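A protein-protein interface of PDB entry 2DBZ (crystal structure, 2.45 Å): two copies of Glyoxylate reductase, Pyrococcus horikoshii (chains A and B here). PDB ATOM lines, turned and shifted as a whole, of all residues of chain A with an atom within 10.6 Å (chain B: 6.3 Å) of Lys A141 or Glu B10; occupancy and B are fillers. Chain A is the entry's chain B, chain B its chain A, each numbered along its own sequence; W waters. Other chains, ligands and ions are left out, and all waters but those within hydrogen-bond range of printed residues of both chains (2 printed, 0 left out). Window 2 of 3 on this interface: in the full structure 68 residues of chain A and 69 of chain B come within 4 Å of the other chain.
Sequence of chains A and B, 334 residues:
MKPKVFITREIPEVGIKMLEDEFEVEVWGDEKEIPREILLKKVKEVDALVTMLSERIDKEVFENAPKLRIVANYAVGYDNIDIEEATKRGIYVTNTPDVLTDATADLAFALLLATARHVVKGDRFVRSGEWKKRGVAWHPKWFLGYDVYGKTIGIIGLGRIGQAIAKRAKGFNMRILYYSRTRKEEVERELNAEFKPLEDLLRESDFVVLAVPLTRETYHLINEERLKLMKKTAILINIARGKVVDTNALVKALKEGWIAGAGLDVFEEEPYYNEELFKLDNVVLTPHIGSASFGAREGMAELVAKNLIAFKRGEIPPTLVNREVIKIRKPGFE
NH1 of Arg B9 lies within hydrogen-bond range of O of Trp A138, 2.8 Å away.
The guanidinium group (NE) of Arg B297 sits at hydrogen-bond distance from the backbone carbonyl oxygen (O) of Pro A140 (3.0 Å).
The side-chain amino group (NZ) of Lys A141 is in salt-bridge range of the side-chain carboxylate (OE1) of Glu B10 (3.1 Å).
N of Met B52 lies within hydrogen-bond range of OG1 of Thr B8, 3.5 Å away.
A ring nitrogen (NE2) of His A118 is in hydrogen-bond range of the backbone carbonyl oxygen (O) of Leu A144.
Among the printed residues, pairs that only touch across the chains: Trp A138 with Arg B297, His A139 with Arg B297, Pro A140 with Arg B9, Pro A140 with Glu B10, Trp A138 with Met B52, Leu A144 with Arg B297, Pro A140 with Met B52, Pro A140 with Ile B11 and His A139 with Arg B9.
Lys A141 touches just one residue of chain B: Glu B10 (3.1 Å).
Of chain A, only Pro A140 (3.6 Å) and Lys A141 (3.1 Å) come within 4 Å of Glu B10.
Ile B11 touches one residue of chain A.
No residue of chain A comes within 4 Å of Pro B12.
No residue of chain A comes within 4 Å of Gly B29.
Printed residues of chain A within 4 Å of Arg B9: Trp A138 (2.8 Å), His A139 (3.9 Å) and Pro A140 (3.6 Å).
Of the printed residues of chain B, His A139 touches Arg B9 (3.9 Å) and Arg B297 (3.5 Å).
Printed residues of chain A within 4 Å of Arg B297: Trp A138 (3.4 Å), His A139 (3.5 Å), Pro A140 (3.0 Å) and Leu A144 (3.8 Å).
Ile B7 touches none of the printed residues of chain A.
Val A136 touches none of the printed residues of chain B.
The nearest residue of chain B that does not touch Lys A141 is Ile B11 (4.05 Å).
Printed residues of chain B that touch a printed residue of chain A: Arg B9, Glu B10, Ile B11, Met B52 and Arg B297.
Of the 14 printed residues of chain A, 5 touch a printed residue of chain B.
Hydrophobic or aromatic side chains of chain A within 4 Å of the printed part of chain B: Trp A138, His A139, Pro A140 and Leu A144.
Among the printed residues, 12 pairs touch across the chains.
Among the printed residues, Asp or Glu carboxylates within 4 Å of a Lys or Arg side-chain nitrogen of the other chain: Lys A141 with Glu B10 (3.1 Å).
No position is printed for both chains.
Of the 12 pairs that touch across the chains among the printed residues, none has its exchanged pair printed and touching as well.
Water W1 lies within hydrogen-bond range of the side-chain amino group of Lys A141, the side-chain carboxylate of Glu B13 and the backbone carbonyl oxygen of Ile B11.
Water W2 bridges NE1 of Trp A138 and NH1 of Arg B297.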
ATOM      1  N   HIS A 118       9.909 -16.253  26.962  1.00  0.00           N
ATOM      2  CA  HIS A 118      10.763 -15.105  26.694  1.00  0.00           C
ATOM      3  C   HIS A 118      10.490 -13.908  27.596  1.00  0.00           C
ATOM      4  O   HIS A 118      10.476 -12.776  27.087  1.00  0.00           O
ATOM      5  CB  HIS A 118      10.576 -14.643  25.242  1.00  0.00           C
ATOM      6  CG  HIS A 118      10.633 -15.745  24.226  1.00  0.00           C
ATOM      7  ND1 HIS A 118      11.797 -16.417  23.908  1.00  0.00           N
ATOM      8  CD2 HIS A 118       9.659 -16.298  23.460  1.00  0.00           C
ATOM      9  CE1 HIS A 118      11.532 -17.341  22.997  1.00  0.00           C
ATOM     10  NE2 HIS A 118      10.244 -17.290  22.708  1.00  0.00           N
ATOM     11  N   LYS A 121      13.680 -11.409  27.674  1.00  0.00           N
ATOM     12  CA  LYS A 121      13.847 -10.749  26.389  1.00  0.00           C
ATOM     13  C   LYS A 121      12.748  -9.718  26.142  1.00  0.00           C
ATOM     14  O   LYS A 121      13.011  -8.614  25.680  1.00  0.00           O
ATOM     15  CB  LYS A 121      13.839 -11.815  25.298  1.00  0.00           C
ATOM     16  CG  LYS A 121      13.831 -11.306  23.872  1.00  0.00           C
ATOM     17  CD  LYS A 121      13.858 -12.507  22.924  1.00  0.00           C
ATOM     18  CE  LYS A 121      13.684 -12.127  21.454  1.00  0.00           C
ATOM     19  NZ  LYS A 121      13.689 -13.364  20.621  1.00  0.00           N
ATOM     20  N   PHE A 125      13.080  -5.568  25.808  1.00  0.00           N
ATOM     21  CA  PHE A 125      12.418  -4.935  24.670  1.00  0.00           C
ATOM     22  C   PHE A 125      11.551  -3.751  25.076  1.00  0.00           C
ATOM     23  O   PHE A 125      11.549  -2.701  24.400  1.00  0.00           O
ATOM     24  CB  PHE A 125      11.542  -5.969  23.959  1.00  0.00           C
ATOM     25  CG  PHE A 125      10.942  -5.494  22.645  1.00  0.00           C
ATOM     26  CD1 PHE A 125      11.754  -5.185  21.556  1.00  0.00           C
ATOM     27  CD2 PHE A 125       9.561  -5.454  22.472  1.00  0.00           C
ATOM     28  CE1 PHE A 125      11.198  -4.853  20.308  1.00  0.00           C
ATOM     29  CE2 PHE A 125       8.990  -5.123  21.228  1.00  0.00           C
ATOM     30  CZ  PHE A 125       9.815  -4.826  20.144  1.00  0.00           C
ATOM     31  N   ARG A 134       9.735   0.981  17.810  1.00  0.00           N
ATOM     32  CA  ARG A 134       9.204   0.192  16.694  1.00  0.00           C
ATOM     33  C   ARG A 134       7.800   0.582  16.232  1.00  0.00           C
ATOM     34  O   ARG A 134       7.388   0.233  15.122  1.00  0.00           O
ATOM     35  CB  ARG A 134       9.194  -1.290  17.067  1.00  0.00           C
ATOM     36  CG  ARG A 134      10.449  -2.031  16.695  1.00  0.00           C
ATOM     37  CD  ARG A 134      10.167  -3.023  15.576  1.00  0.00           C
ATOM     38  NE  ARG A 134      11.009  -4.208  15.716  1.00  0.00           N
ATOM     39  CZ  ARG A 134      10.829  -5.339  15.042  1.00  0.00           C
ATOM     40  NH1 ARG A 134       9.838  -5.446  14.168  1.00  0.00           N
ATOM     41  NH2 ARG A 134      11.622  -6.380  15.266  1.00  0.00           N
ATOM     42  N   VAL A 136       5.102  -0.661  16.884  1.00  0.00           N
ATOM     43  CA  VAL A 136       4.188  -1.798  16.809  1.00  0.00           C
ATOM     44  C   VAL A 136       3.682  -2.172  18.193  1.00  0.00           C
ATOM     45  O   VAL A 136       4.466  -2.419  19.119  1.00  0.00           O
ATOM     46  CB  VAL A 136       4.841  -3.047  16.232  1.00  0.00           C
ATOM     47  CG1 VAL A 136       3.800  -4.155  16.159  1.00  0.00           C
ATOM     48  CG2 VAL A 136       5.429  -2.757  14.859  1.00  0.00           C
ATOM     49  N   ALA A 137       2.362  -2.246  18.311  1.00  0.00           N
ATOM     50  CA  ALA A 137       1.720  -2.574  19.571  1.00  0.00           C
ATOM     51  C   ALA A 137       1.610  -4.074  19.867  1.00  0.00           C
ATOM     52  O   ALA A 137       2.193  -4.589  20.833  1.00  0.00           O
ATOM     53  CB  ALA A 137       0.346  -1.955  19.594  1.00  0.00           C
ATOM     54  N   TRP A 138       0.860  -4.766  19.020  1.00  0.00           N
ATOM     55  CA  TRP A 138       0.608  -6.184  19.186  1.00  0.00           C
ATOM     56  C   TRP A 138       0.720  -6.823  17.816  1.00  0.00           C
ATOM     57  O   TRP A 138       0.205  -6.288  16.839  1.00  0.00           O
ATOM     58  CB  TRP A 138      -0.819  -6.363  19.729  1.00  0.00           C
ATOM     59  CG  TRP A 138      -1.189  -7.746  20.163  1.00  0.00           C
ATOM     60  CD1 TRP A 138      -1.080  -8.270  21.424  1.00  0.00           C
ATOM     61  CD2 TRP A 138      -1.716  -8.792  19.341  1.00  0.00           C
ATOM     62  NE1 TRP A 138      -1.515  -9.578  21.435  1.00  0.00           N
ATOM     63  CE2 TRP A 138      -1.913  -9.922  20.172  1.00  0.00           C
ATOM     64  CE3 TRP A 138      -2.048  -8.885  17.986  1.00  0.00           C
ATOM     65  CZ2 TRP A 138      -2.423 -11.128  19.690  1.00  0.00           C
ATOM     66  CZ3 TRP A 138      -2.556 -10.084  17.505  1.00  0.00           C
ATOM     67  CH2 TRP A 138      -2.734 -11.193  18.355  1.00  0.00           C
ATOM     68  N   HIS A 139       1.388  -7.967  17.745  1.00  0.00           N
ATOM     69  CA  HIS A 139       1.565  -8.683  16.483  1.00  0.00           C
ATOM     70  C   HIS A 139       1.347 -10.198  16.672  1.00  0.00           C
ATOM     71  O   HIS A 139       1.934 -10.791  17.574  1.00  0.00           O
ATOM     72  CB  HIS A 139       2.971  -8.425  15.931  1.00  0.00           C
ATOM     73  CG  HIS A 139       3.170  -8.966  14.555  1.00  0.00           C
ATOM     74  ND1 HIS A 139       3.153  -8.166  13.432  1.00  0.00           N
ATOM     75  CD2 HIS A 139       3.320 -10.236  14.111  1.00  0.00           C
ATOM     76  CE1 HIS A 139       3.284  -8.920  12.355  1.00  0.00           C
ATOM     77  NE2 HIS A 139       3.387 -10.180  12.740  1.00  0.00           N
ATOM     78  N   PRO A 140       0.528 -10.844  15.814  1.00  0.00           N
ATOM     79  CA  PRO A 140       0.237 -12.281  15.893  1.00  0.00           C
ATOM     80  C   PRO A 140       1.426 -13.229  16.057  1.00  0.00           C
ATOM     81  O   PRO A 140       1.315 -14.275  16.717  1.00  0.00           O
ATOM     82  CB  PRO A 140      -0.526 -12.560  14.595  1.00  0.00           C
ATOM     83  CG  PRO A 140      -1.274 -11.310  14.379  1.00  0.00           C
ATOM     84  CD  PRO A 140      -0.218 -10.242  14.690  1.00  0.00           C
ATOM     85  N   LYS A 141       2.560 -12.855  15.471  1.00  0.00           N
ATOM     86  CA  LYS A 141       3.745 -13.697  15.502  1.00  0.00           C
ATOM     87  C   LYS A 141       4.935 -13.185  16.315  1.00  0.00           C
ATOM     88  O   LYS A 141       6.071 -13.638  16.105  1.00  0.00           O
ATOM     89  CB  LYS A 141       4.197 -13.976  14.062  1.00  0.00           C
ATOM     90  CG  LYS A 141       3.124 -14.595  13.166  1.00  0.00           C
ATOM     91  CD  LYS A 141       3.678 -14.882  11.775  1.00  0.00           C
ATOM     92  CE  LYS A 141       2.593 -15.448  10.874  1.00  0.00           C
ATOM     93  NZ  LYS A 141       3.041 -15.621   9.468  1.00  0.00           N
ATOM     94  N   TRP A 142       4.698 -12.255  17.234  1.00  0.00           N
ATOM     95  CA  TRP A 142       5.789 -11.731  18.069  1.00  0.00           C
ATOM     96  C   TRP A 142       6.022 -12.522  19.375  1.00  0.00           C
ATOM     97  O   TRP A 142       5.077 -12.932  20.069  1.00  0.00           O
ATOM     98  CB  TRP A 142       5.545 -10.240  18.398  1.00  0.00           C
ATOM     99  CG  TRP A 142       6.034  -9.281  17.330  1.00  0.00           C
ATOM    100  CD1 TRP A 142       6.251  -9.564  16.008  1.00  0.00           C
ATOM    101  CD2 TRP A 142       6.334  -7.891  17.494  1.00  0.00           C
ATOM    102  NE1 TRP A 142       6.670  -8.441  15.347  1.00  0.00           N
ATOM    103  CE2 TRP A 142       6.731  -7.398  16.231  1.00  0.00           C
ATOM    104  CE3 TRP A 142       6.309  -7.014  18.584  1.00  0.00           C
ATOM    105  CZ2 TRP A 142       7.100  -6.061  16.029  1.00  0.00           C
ATOM    106  CZ3 TRP A 142       6.677  -5.690  18.384  1.00  0.00           C
ATOM    107  CH2 TRP A 142       7.067  -5.225  17.115  1.00  0.00           C
ATOM    108  N   PHE A 143       7.295 -12.738  19.685  1.00  0.00           N
ATOM    109  CA  PHE A 143       7.695 -13.431  20.900  1.00  0.00           C
ATOM    110  C   PHE A 143       6.984 -14.768  21.120  1.00  0.00           C
ATOM    111  O   PHE A 143       6.743 -15.174  22.251  1.00  0.00           O
ATOM    112  CB  PHE A 143       7.467 -12.506  22.102  1.00  0.00           C
ATOM    113  CG  PHE A 143       8.299 -11.251  22.065  1.00  0.00           C
ATOM    114  CD1 PHE A 143       9.616 -11.251  22.520  1.00  0.00           C
ATOM    115  CD2 PHE A 143       7.770 -10.071  21.547  1.00  0.00           C
ATOM    116  CE1 PHE A 143      10.402 -10.076  22.456  1.00  0.00           C
ATOM    117  CE2 PHE A 143       8.527  -8.899  21.475  1.00  0.00           C
ATOM    118  CZ  PHE A 143       9.851  -8.898  21.931  1.00  0.00           C
ATOM    119  N   LEU A 144       6.657 -15.459  20.041  1.00  0.00           N
ATOM    120  CA  LEU A 144       5.993 -16.746  20.163  1.00  0.00           C
ATOM    121  C   LEU A 144       6.803 -17.686  21.039  1.00  0.00           C
ATOM    122  O   LEU A 144       7.977 -17.906  20.780  1.00  0.00           O
ATOM    123  CB  LEU A 144       5.795 -17.359  18.778  1.00  0.00           C
ATOM    124  CG  LEU A 144       4.390 -17.260  18.170  1.00  0.00           C
ATOM    125  CD1 LEU A 144       3.628 -16.022  18.674  1.00  0.00           C
ATOM    126  CD2 LEU A 144       4.541 -17.231  16.663  1.00  0.00           C
ATOM    127  N   GLY A 145       6.178 -18.234  22.079  1.00  0.00           N
ATOM    128  CA  GLY A 145       6.884 -19.157  22.946  1.00  0.00           C
ATOM    129  C   GLY A 145       6.198 -20.507  23.004  1.00  0.00           C
ATOM    130  O   GLY A 145       5.211 -20.751  22.313  1.00  0.00           O
ATOM    131  N   ILE B   7      -7.963  -9.492   6.454  1.00  0.00           N
ATOM    132  CA  ILE B   7      -7.337  -9.679   7.769  1.00  0.00           C
ATOM    133  C   ILE B   7      -6.349  -8.524   7.940  1.00  0.00           C
ATOM    134  O   ILE B   7      -5.493  -8.295   7.086  1.00  0.00           O
ATOM    135  CB  ILE B   7      -6.567 -11.035   7.867  1.00  0.00           C
ATOM    136  CG1 ILE B   7      -7.539 -12.220   7.859  1.00  0.00           C
ATOM    137  CG2 ILE B   7      -5.774 -11.093   9.164  1.00  0.00           C
ATOM    138  CD1 ILE B   7      -8.309 -12.392   6.596  1.00  0.00           C
ATOM    139  N   THR B   8      -6.461  -7.807   9.049  1.00  0.00           N
ATOM    140  CA  THR B   8      -5.611  -6.649   9.288  1.00  0.00           C
ATOM    141  C   THR B   8      -4.173  -6.947   9.704  1.00  0.00           C
ATOM    142  O   THR B   8      -3.368  -6.032   9.905  1.00  0.00           O
ATOM    143  CB  THR B   8      -6.271  -5.705  10.329  1.00  0.00           C
ATOM    144  OG1 THR B   8      -6.487  -6.415  11.560  1.00  0.00           O
ATOM    145  CG2 THR B   8      -7.609  -5.194   9.797  1.00  0.00           C
ATOM    146  N   ARG B   9      -3.830  -8.218   9.854  1.00  0.00           N
ATOM    147  CA  ARG B   9      -2.448  -8.532  10.216  1.00  0.00           C
ATOM    148  C   ARG B   9      -2.189  -9.981   9.857  1.00  0.00           C
ATOM    149  O   ARG B   9      -3.113 -10.780   9.804  1.00  0.00           O
ATOM    150  CB  ARG B   9      -2.192  -8.283  11.715  1.00  0.00           C
ATOM    151  CG  ARG B   9      -0.744  -7.907  12.027  1.00  0.00           C
ATOM    152  CD  ARG B   9      -0.479  -6.464  11.614  1.00  0.00           C
ATOM    153  NE  ARG B   9      -1.274  -5.605  12.469  1.00  0.00           N
ATOM    154  CZ  ARG B   9      -0.873  -5.168  13.659  1.00  0.00           C
ATOM    155  NH1 ARG B   9       0.337  -5.485  14.118  1.00  0.00           N
ATOM    156  NH2 ARG B   9      -1.713  -4.486  14.430  1.00  0.00           N
ATOM    157  N   GLU B  10      -0.939 -10.330   9.606  1.00  0.00           N
ATOM    158  CA  GLU B  10      -0.661 -11.704   9.230  1.00  0.00           C
ATOM    159  C   GLU B  10      -0.793 -12.750  10.362  1.00  0.00           C
ATOM    160  O   GLU B  10       0.155 -13.020  11.095  1.00  0.00           O
ATOM    161  CB  GLU B  10       0.721 -11.789   8.595  1.00  0.00           C
ATOM    162  CG  GLU B  10       0.949 -13.100   7.883  1.00  0.00           C
ATOM    163  CD  GLU B  10       2.300 -13.151   7.203  1.00  0.00           C
ATOM    164  OE1 GLU B  10       3.328 -12.980   7.911  1.00  0.00           O
ATOM    165  OE2 GLU B  10       2.327 -13.369   5.964  1.00  0.00           O
ATOM    166  N   ILE B  11      -1.975 -13.332  10.497  1.00  0.00           N
ATOM    167  CA  ILE B  11      -2.186 -14.352  11.503  1.00  0.00           C
ATOM    168  C   ILE B  11      -1.561 -15.618  10.961  1.00  0.00           C
ATOM    169  O   ILE B  11      -1.290 -15.704   9.764  1.00  0.00           O
ATOM    170  CB  ILE B  11      -3.678 -14.611  11.736  1.00  0.00           C
ATOM    171  CG1 ILE B  11      -4.327 -15.073  10.431  1.00  0.00           C
ATOM    172  CG2 ILE B  11      -4.349 -13.344  12.229  1.00  0.00           C
ATOM    173  CD1 ILE B  11      -5.826 -15.321  10.542  1.00  0.00           C
ATOM    174  N   PRO B  12      -1.316 -16.616  11.839  1.00  0.00           N
ATOM    175  CA  PRO B  12      -0.722 -17.903  11.469  1.00  0.00           C
ATOM    176  C   PRO B  12      -1.371 -18.389  10.189  1.00  0.00           C
ATOM    177  O   PRO B  12      -2.589 -18.285  10.029  1.00  0.00           O
ATOM    178  CB  PRO B  12      -1.058 -18.777  12.670  1.00  0.00           C
ATOM    179  CG  PRO B  12      -0.835 -17.825  13.800  1.00  0.00           C
ATOM    180  CD  PRO B  12      -1.534 -16.554  13.296  1.00  0.00           C
ATOM    181  N   GLU B  13      -0.544 -18.901   9.279  1.00  0.00           N
ATOM    182  CA  GLU B  13      -0.995 -19.382   7.978  1.00  0.00           C
ATOM    183  C   GLU B  13      -2.127 -20.430   8.002  1.00  0.00           C
ATOM    184  O   GLU B  13      -2.929 -20.482   7.071  1.00  0.00           O
ATOM    185  CB  GLU B  13       0.216 -19.926   7.192  1.00  0.00           C
ATOM    186  CG  GLU B  13       0.065 -19.916   5.643  1.00  0.00           C
ATOM    187  CD  GLU B  13      -0.077 -18.503   5.049  1.00  0.00           C
ATOM    188  OE1 GLU B  13       0.605 -17.559   5.518  1.00  0.00           O
ATOM    189  OE2 GLU B  13      -0.871 -18.340   4.096  1.00  0.00           O
ATOM    190  N   ILE B  16      -5.448 -18.714   7.486  1.00  0.00           N
ATOM    191  CA  ILE B  16      -5.557 -18.206   6.115  1.00  0.00           C
ATOM    192  C   ILE B  16      -5.921 -19.349   5.169  1.00  0.00           C
ATOM    193  O   ILE B  16      -6.855 -19.235   4.376  1.00  0.00           O
ATOM    194  CB  ILE B  16      -4.213 -17.572   5.612  1.00  0.00           C
ATOM    195  CG1 ILE B  16      -3.900 -16.292   6.378  1.00  0.00           C
ATOM    196  CG2 ILE B  16      -4.302 -17.271   4.102  1.00  0.00           C
ATOM    197  CD1 ILE B  16      -2.577 -15.678   5.997  1.00  0.00           C
ATOM    198  N   VAL B  27      -4.679  -9.890   3.044  1.00  0.00           N
ATOM    199  CA  VAL B  27      -4.104  -9.702   4.367  1.00  0.00           C
ATOM    200  C   VAL B  27      -3.110  -8.536   4.427  1.00  0.00           C
ATOM    201  O   VAL B  27      -2.231  -8.434   3.582  1.00  0.00           O
ATOM    202  CB  VAL B  27      -3.361 -10.983   4.791  1.00  0.00           C
ATOM    203  CG1 VAL B  27      -2.900 -10.870   6.227  1.00  0.00           C
ATOM    204  CG2 VAL B  27      -4.251 -12.190   4.580  1.00  0.00           C
ATOM    205  N   TRP B  28      -3.234  -7.666   5.426  1.00  0.00           N
ATOM    206  CA  TRP B  28      -2.286  -6.555   5.573  1.00  0.00           C
ATOM    207  C   TRP B  28      -0.919  -7.183   5.899  1.00  0.00           C
ATOM    208  O   TRP B  28      -0.792  -7.972   6.842  1.00  0.00           O
ATOM    209  CB  TRP B  28      -2.758  -5.610   6.691  1.00  0.00           C
ATOM    210  CG  TRP B  28      -1.830  -4.462   6.993  1.00  0.00           C
ATOM    211  CD1 TRP B  28      -1.047  -4.314   8.102  1.00  0.00           C
ATOM    212  CD2 TRP B  28      -1.567  -3.319   6.162  1.00  0.00           C
ATOM    213  NE1 TRP B  28      -0.315  -3.155   8.018  1.00  0.00           N
ATOM    214  CE2 TRP B  28      -0.614  -2.523   6.838  1.00  0.00           C
ATOM    215  CE3 TRP B  28      -2.042  -2.892   4.915  1.00  0.00           C
ATOM    216  CZ2 TRP B  28      -0.120  -1.322   6.303  1.00  0.00           C
ATOM    217  CZ3 TRP B  28      -1.549  -1.694   4.383  1.00  0.00           C
ATOM    218  CH2 TRP B  28      -0.597  -0.928   5.079  1.00  0.00           C
ATOM    219  N   GLY B  29       0.102  -6.833   5.119  1.00  0.00           N
ATOM    220  CA  GLY B  29       1.423  -7.426   5.291  1.00  0.00           C
ATOM    221  C   GLY B  29       2.464  -6.705   6.112  1.00  0.00           C
ATOM    222  O   GLY B  29       3.513  -7.276   6.399  1.00  0.00           O
ATOM    223  N   ASP B  30       2.217  -5.457   6.486  1.00  0.00           N
ATOM    224  CA  ASP B  30       3.205  -4.755   7.303  1.00  0.00           C
ATOM    225  C   ASP B  30       3.074  -5.232   8.749  1.00  0.00           C
ATOM    226  O   ASP B  30       2.030  -5.758   9.135  1.00  0.00           O
ATOM    227  CB  ASP B  30       2.984  -3.247   7.230  1.00  0.00           C
ATOM    228  CG  ASP B  30       4.145  -2.477   7.801  1.00  0.00           C
ATOM    229  OD1 ASP B  30       4.117  -2.128   9.003  1.00  0.00           O
ATOM    230  OD2 ASP B  30       5.108  -2.238   7.041  1.00  0.00           O
ATOM    231  N   MET B  52      -7.398  -7.005  14.887  1.00  0.00           N
ATOM    232  CA  MET B  52      -6.525  -7.250  16.037  1.00  0.00           C
ATOM    233  C   MET B  52      -6.955  -6.353  17.213  1.00  0.00           C
ATOM    234  O   MET B  52      -7.765  -5.437  17.043  1.00  0.00           O
ATOM    235  CB  MET B  52      -5.073  -6.907  15.677  1.00  0.00           C
ATOM    236  CG  MET B  52      -4.554  -7.566  14.422  1.00  0.00           C
ATOM    237  SD  MET B  52      -4.508  -9.335  14.515  1.00  0.00           S
ATOM    238  CE  MET B  52      -5.559  -9.789  13.156  1.00  0.00           C
ATOM    239  N   ARG B 297      -1.734 -19.156  19.448  1.00  0.00           N
ATOM    240  CA  ARG B 297      -1.899 -18.328  18.251  1.00  0.00           C
ATOM    241  C   ARG B 297      -2.389 -19.143  17.082  1.00  0.00           C
ATOM    242  O   ARG B 297      -3.128 -18.639  16.234  1.00  0.00           O
ATOM    243  CB  ARG B 297      -0.605 -17.608  17.877  1.00  0.00           C
ATOM    244  CG  ARG B 297      -0.084 -16.680  18.956  1.00  0.00           C
ATOM    245  CD  ARG B 297      -0.942 -15.420  19.199  1.00  0.00           C
ATOM    246  NE  ARG B 297      -0.035 -14.268  19.365  1.00  0.00           N
ATOM    247  CZ  ARG B 297      -0.030 -13.440  20.402  1.00  0.00           C
ATOM    248  NH1 ARG B 297      -0.889 -13.601  21.389  1.00  0.00           N
ATOM    249  NH2 ARG B 297       0.848 -12.458  20.459  1.00  0.00           N
HETATM  250  O   HOH W   1       0.833 -16.131   7.899  1.00  0.00           O
HETATM  251  O   HOH W   2      -0.638 -11.343  23.570  1.00  0.00           O
